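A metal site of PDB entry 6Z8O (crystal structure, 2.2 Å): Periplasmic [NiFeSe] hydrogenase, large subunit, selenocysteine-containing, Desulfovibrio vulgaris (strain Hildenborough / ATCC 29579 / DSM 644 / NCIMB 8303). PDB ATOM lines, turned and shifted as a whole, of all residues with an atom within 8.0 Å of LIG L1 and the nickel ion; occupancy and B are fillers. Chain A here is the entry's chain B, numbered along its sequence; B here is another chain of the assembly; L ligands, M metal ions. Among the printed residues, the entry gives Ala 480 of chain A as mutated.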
ATOM      1  N   ILE A  16      -9.160   1.952 -16.004  1.00  0.00           N
ATOM      2  CA  ILE A  16      -8.095   0.975 -15.845  1.00  0.00           C
ATOM      3  C   ILE A  16      -8.186   0.118 -17.105  1.00  0.00           C
ATOM      4  O   ILE A  16      -8.985   0.404 -17.997  1.00  0.00           O
ATOM      5  CB  ILE A  16      -8.265   0.111 -14.589  1.00  0.00           C
ATOM      6  CG1 ILE A  16      -9.561  -0.703 -14.634  1.00  0.00           C
ATOM      7  CG2 ILE A  16      -8.222   0.991 -13.357  1.00  0.00           C
ATOM      8  CD1 ILE A  16      -9.622  -1.867 -13.638  1.00  0.00           C
ATOM      9  N   GLU A  17      -7.411  -0.945 -17.165  1.00  0.00           N
ATOM     10  CA  GLU A  17      -7.570  -1.959 -18.194  1.00  0.00           C
ATOM     11  C   GLU A  17      -8.164  -3.190 -17.536  1.00  0.00           C
ATOM     12  O   GLU A  17      -7.519  -3.826 -16.692  1.00  0.00           O
ATOM     13  CB  GLU A  17      -6.252  -2.291 -18.878  1.00  0.00           C
ATOM     14  CG  GLU A  17      -6.388  -3.299 -20.028  1.00  0.00           C
ATOM     15  CD  GLU A  17      -6.848  -4.686 -19.578  1.00  0.00           C
ATOM     16  OE1 GLU A  17      -6.342  -5.187 -18.556  1.00  0.00           O
ATOM     17  OE2 GLU A  17      -7.737  -5.267 -20.228  1.00  0.00           O
ATOM     18  N   GLN A  61       0.646 -12.365 -26.447  1.00  0.00           N
ATOM     19  CA  GLN A  61       0.371 -10.931 -26.524  1.00  0.00           C
ATOM     20  C   GLN A  61      -1.126 -10.662 -26.394  1.00  0.00           C
ATOM     21  O   GLN A  61      -1.514  -9.620 -25.871  1.00  0.00           O
ATOM     22  CB  GLN A  61       0.878 -10.348 -27.829  1.00  0.00           C
ATOM     23  CG  GLN A  61       2.291 -10.707 -28.237  1.00  0.00           C
ATOM     24  CD  GLN A  61       2.781  -9.795 -29.346  1.00  0.00           C
ATOM     25  OE1 GLN A  61       2.997  -8.613 -29.128  1.00  0.00           O
ATOM     26  NE2 GLN A  61       2.870 -10.336 -30.559  1.00  0.00           N
ATOM     27  N   ILE A  63      -3.089 -11.775 -24.433  1.00  0.00           N
ATOM     28  CA  ILE A  63      -3.399 -11.591 -23.025  1.00  0.00           C
ATOM     29  C   ILE A  63      -3.840 -10.150 -22.784  1.00  0.00           C
ATOM     30  O   ILE A  63      -4.947  -9.907 -22.301  1.00  0.00           O
ATOM     31  CB  ILE A  63      -2.172 -11.988 -22.174  1.00  0.00           C
ATOM     32  CG1 ILE A  63      -2.085 -13.520 -22.110  1.00  0.00           C
ATOM     33  CG2 ILE A  63      -2.217 -11.352 -20.791  1.00  0.00           C
ATOM     34  CD1 ILE A  63      -0.788 -14.037 -21.544  1.00  0.00           C
ATOM     35  N   CYS A  64      -2.972  -9.208 -23.138  1.00  0.00           N
ATOM     36  CA  CYS A  64      -3.219  -7.790 -22.946  1.00  0.00           C
ATOM     37  C   CYS A  64      -2.914  -6.965 -24.199  1.00  0.00           C
ATOM     38  O   CYS A  64      -1.938  -7.164 -24.925  1.00  0.00           O
ATOM     39  CB  CYS A  64      -2.373  -7.254 -21.784  1.00  0.00           C
ATOM     40  SG  CYS A  64      -3.035  -5.790 -21.103  1.00  0.00           S
ATOM     41  N   GLY A  65      -3.796  -6.003 -24.466  1.00  0.00           N
ATOM     42  CA  GLY A  65      -3.675  -5.176 -25.651  1.00  0.00           C
ATOM     43  C   GLY A  65      -2.841  -3.922 -25.458  1.00  0.00           C
ATOM     44  O   GLY A  65      -2.452  -3.256 -26.416  1.00  0.00           O
ATOM     45  N   VAL A  66      -2.546  -3.608 -24.195  1.00  0.00           N
ATOM     46  CA  VAL A  66      -1.814  -2.400 -23.849  1.00  0.00           C
ATOM     47  C   VAL A  66      -0.317  -2.665 -23.788  1.00  0.00           C
ATOM     48  O   VAL A  66       0.487  -1.865 -24.272  1.00  0.00           O
ATOM     49  CB  VAL A  66      -2.331  -1.872 -22.487  1.00  0.00           C
ATOM     50  CG1 VAL A  66      -1.446  -0.739 -21.968  1.00  0.00           C
ATOM     51  CG2 VAL A  66      -3.770  -1.426 -22.607  1.00  0.00           C
ATOM     52  N   CYS A  67       0.044  -3.791 -23.190  1.00  0.00           N
ATOM     53  CA  CYS A  67       1.413  -4.207 -22.936  1.00  0.00           C
ATOM     54  C   CYS A  67       1.726  -5.534 -23.620  1.00  0.00           C
ATOM     55  O   CYS A  67       2.252  -6.446 -22.976  1.00  0.00           O
ATOM     56  CB  CYS A  67       1.623  -4.338 -21.426  1.00  0.00           C
ATOM     57  SG  CYS A  67       0.551  -5.608 -20.707  1.00  0.00           S
ATOM     58  N   PRO A  68       1.423  -5.692 -24.911  1.00  0.00           N
ATOM     59  CA  PRO A  68       1.750  -6.954 -25.575  1.00  0.00           C
ATOM     60  C   PRO A  68       3.247  -7.185 -25.754  1.00  0.00           C
ATOM     61  O   PRO A  68       3.680  -8.340 -25.740  1.00  0.00           O
ATOM     62  CB  PRO A  68       1.015  -6.849 -26.912  1.00  0.00           C
ATOM     63  CG  PRO A  68       0.916  -5.401 -27.177  1.00  0.00           C
ATOM     64  CD  PRO A  68       0.733  -4.762 -25.828  1.00  0.00           C
ATOM     65  N   ALA A  70       5.655  -6.423 -23.716  1.00  0.00           N
ATOM     66  CA  ALA A  70       6.167  -7.013 -22.486  1.00  0.00           C
ATOM     67  C   ALA A  70       5.942  -8.523 -22.478  1.00  0.00           C
ATOM     68  O   ALA A  70       6.769  -9.276 -21.955  1.00  0.00           O
ATOM     69  CB  ALA A  70       5.515  -6.372 -21.266  1.00  0.00           C
ATOM     70  N   HIS A  71       4.830  -8.971 -23.067  1.00  0.00           N
ATOM     71  CA  HIS A  71       4.555 -10.407 -23.146  1.00  0.00           C
ATOM     72  C   HIS A  71       5.373 -11.071 -24.243  1.00  0.00           C
ATOM     73  O   HIS A  71       6.013 -12.101 -23.996  1.00  0.00           O
ATOM     74  CB  HIS A  71       3.063 -10.638 -23.374  1.00  0.00           C
ATOM     75  CG  HIS A  71       2.241 -10.471 -22.134  1.00  0.00           C
ATOM     76  ND1 HIS A  71       2.349 -11.335 -21.061  1.00  0.00           N
ATOM     77  CD2 HIS A  71       1.313  -9.550 -21.780  1.00  0.00           C
ATOM     78  CE1 HIS A  71       1.514 -10.949 -20.108  1.00  0.00           C
ATOM     79  NE2 HIS A  71       0.874  -9.873 -20.524  1.00  0.00           N
ATOM     80  N   ASN A 102       7.032   1.429 -26.112  1.00  0.00           N
ATOM     81  CA  ASN A 102       5.698   1.219 -25.576  1.00  0.00           C
ATOM     82  C   ASN A 102       5.615   1.497 -24.077  1.00  0.00           C
ATOM     83  O   ASN A 102       4.536   1.845 -23.584  1.00  0.00           O
ATOM     84  CB  ASN A 102       5.229  -0.212 -25.827  1.00  0.00           C
ATOM     85  CG  ASN A 102       3.732  -0.357 -25.714  1.00  0.00           C
ATOM     86  OD1 ASN A 102       2.964   0.426 -26.279  1.00  0.00           O
ATOM     87  ND2 ASN A 102       3.294  -1.327 -24.918  1.00  0.00           N
ATOM     88  N   SER A 106       2.694   3.424 -22.899  1.00  0.00           N
ATOM     89  CA  SER A 106       1.866   2.979 -21.788  1.00  0.00           C
ATOM     90  C   SER A 106       1.770   4.050 -20.707  1.00  0.00           C
ATOM     91  O   SER A 106       0.670   4.388 -20.253  1.00  0.00           O
ATOM     92  CB  SER A 106       2.444   1.676 -21.212  1.00  0.00           C
ATOM     93  OG  SER A 106       1.899   1.410 -19.931  1.00  0.00           O
ATOM     94  N   LEU A 109      -0.194   7.056 -21.748  1.00  0.00           N
ATOM     95  CA  LEU A 109      -1.594   6.634 -21.782  1.00  0.00           C
ATOM     96  C   LEU A 109      -2.189   6.608 -20.385  1.00  0.00           C
ATOM     97  O   LEU A 109      -3.270   7.153 -20.150  1.00  0.00           O
ATOM     98  CB  LEU A 109      -1.702   5.262 -22.439  1.00  0.00           C
ATOM     99  CG  LEU A 109      -3.077   4.584 -22.379  1.00  0.00           C
ATOM    100  CD1 LEU A 109      -3.956   5.065 -23.514  1.00  0.00           C
ATOM    101  CD2 LEU A 109      -2.917   3.072 -22.398  1.00  0.00           C
ATOM    102  N   LEU A 114      -6.167   7.667 -18.503  1.00  0.00           N
ATOM    103  CA  LEU A 114      -6.747   6.871 -17.428  1.00  0.00           C
ATOM    104  C   LEU A 114      -6.845   7.659 -16.121  1.00  0.00           C
ATOM    105  O   LEU A 114      -7.949   7.838 -15.600  1.00  0.00           O
ATOM    106  CB  LEU A 114      -5.929   5.567 -17.253  1.00  0.00           C
ATOM    107  CG  LEU A 114      -5.902   4.647 -18.480  1.00  0.00           C
ATOM    108  CD1 LEU A 114      -5.048   3.404 -18.265  1.00  0.00           C
ATOM    109  CD2 LEU A 114      -7.309   4.211 -18.885  1.00  0.00           C
ATOM    110  N   ALA A 409       7.449  -5.544 -17.355  1.00  0.00           N
ATOM    111  CA  ALA A 409       6.400  -4.853 -18.079  1.00  0.00           C
ATOM    112  C   ALA A 409       6.253  -3.428 -17.541  1.00  0.00           C
ATOM    113  O   ALA A 409       6.726  -3.114 -16.446  1.00  0.00           O
ATOM    114  CB  ALA A 409       5.083  -5.609 -17.932  1.00  0.00           C
ATOM    115  N   PRO A 410       5.604  -2.538 -18.300  1.00  0.00           N
ATOM    116  CA  PRO A 410       5.370  -1.174 -17.809  1.00  0.00           C
ATOM    117  C   PRO A 410       4.779  -1.128 -16.411  1.00  0.00           C
ATOM    118  O   PRO A 410       5.025  -0.160 -15.677  1.00  0.00           O
ATOM    119  CB  PRO A 410       4.396  -0.595 -18.829  1.00  0.00           C
ATOM    120  CG  PRO A 410       4.623  -1.366 -20.072  1.00  0.00           C
ATOM    121  CD  PRO A 410       5.122  -2.726 -19.683  1.00  0.00           C
ATOM    122  N   ARG A 411       4.008  -2.143 -16.022  1.00  0.00           N
ATOM    123  CA  ARG A 411       3.334  -2.149 -14.731  1.00  0.00           C
ATOM    124  C   ARG A 411       4.046  -2.993 -13.684  1.00  0.00           C
ATOM    125  O   ARG A 411       3.573  -3.054 -12.543  1.00  0.00           O
ATOM    126  CB  ARG A 411       1.895  -2.644 -14.906  1.00  0.00           C
ATOM    127  CG  ARG A 411       0.959  -1.571 -15.429  1.00  0.00           C
ATOM    128  CD  ARG A 411      -0.180  -2.154 -16.239  1.00  0.00           C
ATOM    129  NE  ARG A 411      -0.898  -1.124 -16.993  1.00  0.00           N
ATOM    130  CZ  ARG A 411      -0.448  -0.532 -18.095  1.00  0.00           C
ATOM    131  NH1 ARG A 411       0.749  -0.856 -18.583  1.00  0.00           N
ATOM    132  NH2 ARG A 411      -1.180   0.386 -18.710  1.00  0.00           N
ATOM    133  N   SER A 432       2.579 -12.064 -13.724  1.00  0.00           N
ATOM    134  CA  SER A 432       2.573 -10.807 -14.456  1.00  0.00           C
ATOM    135  C   SER A 432       2.410  -9.650 -13.480  1.00  0.00           C
ATOM    136  O   SER A 432       2.085  -9.834 -12.298  1.00  0.00           O
ATOM    137  CB  SER A 432       1.477 -10.800 -15.529  1.00  0.00           C
ATOM    138  OG  SER A 432       0.203 -11.081 -14.967  1.00  0.00           O
ATOM    139  N   ALA A 433       2.642  -8.444 -13.983  1.00  0.00           N
ATOM    140  CA  ALA A 433       2.775  -7.287 -13.101  1.00  0.00           C
ATOM    141  C   ALA A 433       1.532  -7.084 -12.253  1.00  0.00           C
ATOM    142  O   ALA A 433       1.585  -7.152 -11.025  1.00  0.00           O
ATOM    143  CB  ALA A 433       3.081  -6.042 -13.937  1.00  0.00           C
ATOM    144  N   SER A 434       0.389  -6.822 -12.899  1.00  0.00           N
ATOM    145  CA  SER A 434      -0.878  -6.641 -12.190  1.00  0.00           C
ATOM    146  C   SER A 434      -1.269  -7.834 -11.330  1.00  0.00           C
ATOM    147  O   SER A 434      -2.230  -7.734 -10.566  1.00  0.00           O
ATOM    148  CB  SER A 434      -1.996  -6.354 -13.188  1.00  0.00           C
ATOM    149  OG  SER A 434      -1.886  -5.056 -13.734  1.00  0.00           O
ATOM    150  N   ASP A 476      -1.945   1.639 -11.971  1.00  0.00           N
ATOM    151  CA  ASP A 476      -1.941   1.334 -13.397  1.00  0.00           C
ATOM    152  C   ASP A 476      -2.417  -0.091 -13.637  1.00  0.00           C
ATOM    153  O   ASP A 476      -1.745  -0.862 -14.329  1.00  0.00           O
ATOM    154  CB  ASP A 476      -0.534   1.526 -13.966  1.00  0.00           C
ATOM    155  CG  ASP A 476      -0.512   1.532 -15.479  1.00  0.00           C
ATOM    156  OD1 ASP A 476      -1.559   1.836 -16.099  1.00  0.00           O
ATOM    157  OD2 ASP A 476       0.548   1.235 -16.060  1.00  0.00           O
ATOM    158  N   PRO A 477      -3.592  -0.472 -13.121  1.00  0.00           N
ATOM    159  CA  PRO A 477      -3.950  -1.883 -13.216  1.00  0.00           C
ATOM    160  C   PRO A 477      -4.408  -2.389 -14.585  1.00  0.00           C
ATOM    161  O   PRO A 477      -5.034  -1.667 -15.358  1.00  0.00           O
ATOM    162  CB  PRO A 477      -5.110  -2.029 -12.217  1.00  0.00           C
ATOM    163  CG  PRO A 477      -5.493  -0.641 -11.809  1.00  0.00           C
ATOM    164  CD  PRO A 477      -4.677   0.345 -12.571  1.00  0.00           C
ATOM    165  N   SEC A 478      -4.056  -3.649 -14.820  1.00  0.00           N
ATOM    166  CA  SEC A 478      -4.424  -4.433 -15.976  1.00  0.00           C
ATOM    167  CB  SEC A 478      -3.205  -4.681 -16.864  1.00  0.00           C
ATOM    168 SE   SEC A 478      -3.408  -4.085 -18.719  1.00  0.00          SE
ATOM    169  C   SEC A 478      -4.957  -5.738 -15.472  1.00  0.00           C
ATOM    170  O   SEC A 478      -4.177  -6.609 -15.098  1.00  0.00           O
ATOM    171  N   LEU A 479      -6.275  -5.908 -15.416  1.00  0.00           N
ATOM    172  CA  LEU A 479      -6.799  -7.156 -14.861  1.00  0.00           C
ATOM    173  C   LEU A 479      -6.756  -8.285 -15.881  1.00  0.00           C
ATOM    174  O   LEU A 479      -6.929  -9.452 -15.530  1.00  0.00           O
ATOM    175  CB  LEU A 479      -8.221  -6.949 -14.345  1.00  0.00           C
ATOM    176  CG  LEU A 479      -8.348  -6.426 -12.911  1.00  0.00           C
ATOM    177  CD1 LEU A 479      -7.922  -7.495 -11.904  1.00  0.00           C
ATOM    178  CD2 LEU A 479      -7.508  -5.164 -12.708  1.00  0.00           C
ATOM    179  N   ALA A 480      -6.536  -7.935 -17.147  1.00  0.00           N
ATOM    180  CA  ALA A 480      -6.235  -8.958 -18.146  1.00  0.00           C
ATOM    181  C   ALA A 480      -4.872  -9.582 -17.885  1.00  0.00           C
ATOM    182  O   ALA A 480      -4.719 -10.802 -17.940  1.00  0.00           O
ATOM    183  CB  ALA A 480      -6.292  -8.351 -19.546  1.00  0.00           C
ATOM    184  N   CYS A 481      -3.867  -8.756 -17.577  1.00  0.00           N
ATOM    185  CA  CYS A 481      -2.543  -9.286 -17.252  1.00  0.00           C
ATOM    186  C   CYS A 481      -2.579 -10.075 -15.951  1.00  0.00           C
ATOM    187  O   CYS A 481      -1.882 -11.088 -15.816  1.00  0.00           O
ATOM    188  CB  CYS A 481      -1.526  -8.148 -17.160  1.00  0.00           C
ATOM    189  SG  CYS A 481      -0.787  -7.670 -18.737  1.00  0.00           S
ATOM    190  N   ALA A 482      -3.380  -9.628 -14.988  1.00  0.00           N
ATOM    191  CA  ALA A 482      -3.497 -10.356 -13.722  1.00  0.00           C
ATOM    192  C   ALA A 482      -4.054 -11.757 -13.939  1.00  0.00           C
ATOM    193  O   ALA A 482      -3.461 -12.748 -13.499  1.00  0.00           O
ATOM    194  CB  ALA A 482      -4.361  -9.561 -12.752  1.00  0.00           C
ATOM    195  N   CYS B  18      -8.798  -8.383 -24.733  1.00  0.00           N
ATOM    196  CA  CYS B  18      -7.510  -7.944 -24.232  1.00  0.00           C
ATOM    197  C   CYS B  18      -7.358  -6.429 -24.276  1.00  0.00           C
ATOM    198  O   CYS B  18      -6.233  -5.925 -24.218  1.00  0.00           O
ATOM    199  CB  CYS B  18      -6.390  -8.629 -25.022  1.00  0.00           C
ATOM    200  SG  CYS B  18      -5.959  -7.766 -26.540  1.00  0.00           S
ATOM    201  N   THR B  19      -8.471  -5.703 -24.377  1.00  0.00           N
ATOM    202  CA  THR B  19      -8.474  -4.264 -24.606  1.00  0.00           C
ATOM    203  C   THR B  19      -7.716  -3.882 -25.874  1.00  0.00           C
ATOM    204  O   THR B  19      -7.350  -2.721 -26.074  1.00  0.00           O
ATOM    205  CB  THR B  19      -7.914  -3.512 -23.388  1.00  0.00           C
ATOM    206  OG1 THR B  19      -8.656  -3.882 -22.219  1.00  0.00           O
ATOM    207  CG2 THR B  19      -8.047  -1.998 -23.580  1.00  0.00           C
HETATM  208  S1  LIG L   1      -1.434  -3.516 -19.157  1.00  0.00           S
HETATM  209 FE1  LG2 L   2       0.714  -6.004 -18.467  1.00  0.00          FE
HETATM  210  C1  LG2 L   2       0.352  -5.748 -16.706  1.00  0.00           C
HETATM  211  N1  LG2 L   2       0.181  -5.524 -15.594  1.00  0.00           N
HETATM  212  C2  LG2 L   2       1.707  -4.447 -18.398  1.00  0.00           C
HETATM  213  N2  LG2 L   2       2.368  -3.478 -18.332  1.00  0.00           N
HETATM  214  C3  LG2 L   2       2.161  -6.999 -17.945  1.00  0.00           C
HETATM  215  O1  LG2 L   2       3.052  -7.590 -17.582  1.00  0.00           O
HETATM  216 NI    NI M   1      -1.409  -5.584 -19.479  1.00  0.00          NI
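SE of SEC 478 is covalently linked to S1 of LIG L1 (2.1 Å). A sulfur (S1) of LIG L1 sits close to the guanidinium group of Arg 411 (3.3 Å). An iron atom (FE1) of LG2 L2 is bound by the side-chain sulfur (SG) of Cys 481, at 2.3 Å. SG of Cys 67 is bound to FE1 of LG2 L2 (2.3 Å). N of Arg 411 is in hydrogen-bond range of N2 of LG2 L2. NH1 of Arg 411 is in hydrogen-bond range of N2 of LG2 L2 (3.1 Å). The backbone NH of Ser 434 lies within hydrogen-bond range of a nitrogen (N1) of LG2 L2. A nitrogen (N1) of LG2 L2 sits at hydrogen-bond distance from the side-chain hydroxyl of Ser 434.
The side-chain hydroxyl (OG) of Ser 434 is in hydrogen-bond range of N of SEC 478. SG of Cys 481 sits close to NE2 of His 71, at 3.3 Å. The guanidinium group (NE) of Arg 411 is in salt-bridge range of the side-chain carboxylate (OD2) of Asp 476, 2.9 Å away. The guanidinium group (NH1) of Arg 411 sits at hydrogen-bond distance from the side-chain hydroxyl (OG) of Ser 106, 2.9 Å away. ND2 of Asn 102 sits at hydrogen-bond distance from O of Val 66 (2.9 Å).
Merely in contact with LIG L1: Val 66. Five residues have an atom within 4 Å of LIG L1: Cys 64, Val 66, Cys 67, Arg 411 and SEC 478. The nearest printed residue that does not touch LIG L1 is Cys 481 (4.2 Å).
Within 4 Å of the nickel ion: Cys 64, Cys 67, SEC 478 and Cys 481.
The nickel ion is bound by S1 of LIG L1 (2.1 Å), SG of Cys 481 (2.3 Å), SG of Cys 64 (2.3 Å), SG of Cys 67 (2.3 Å) and SE of SEC 478 (2.6 Å).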
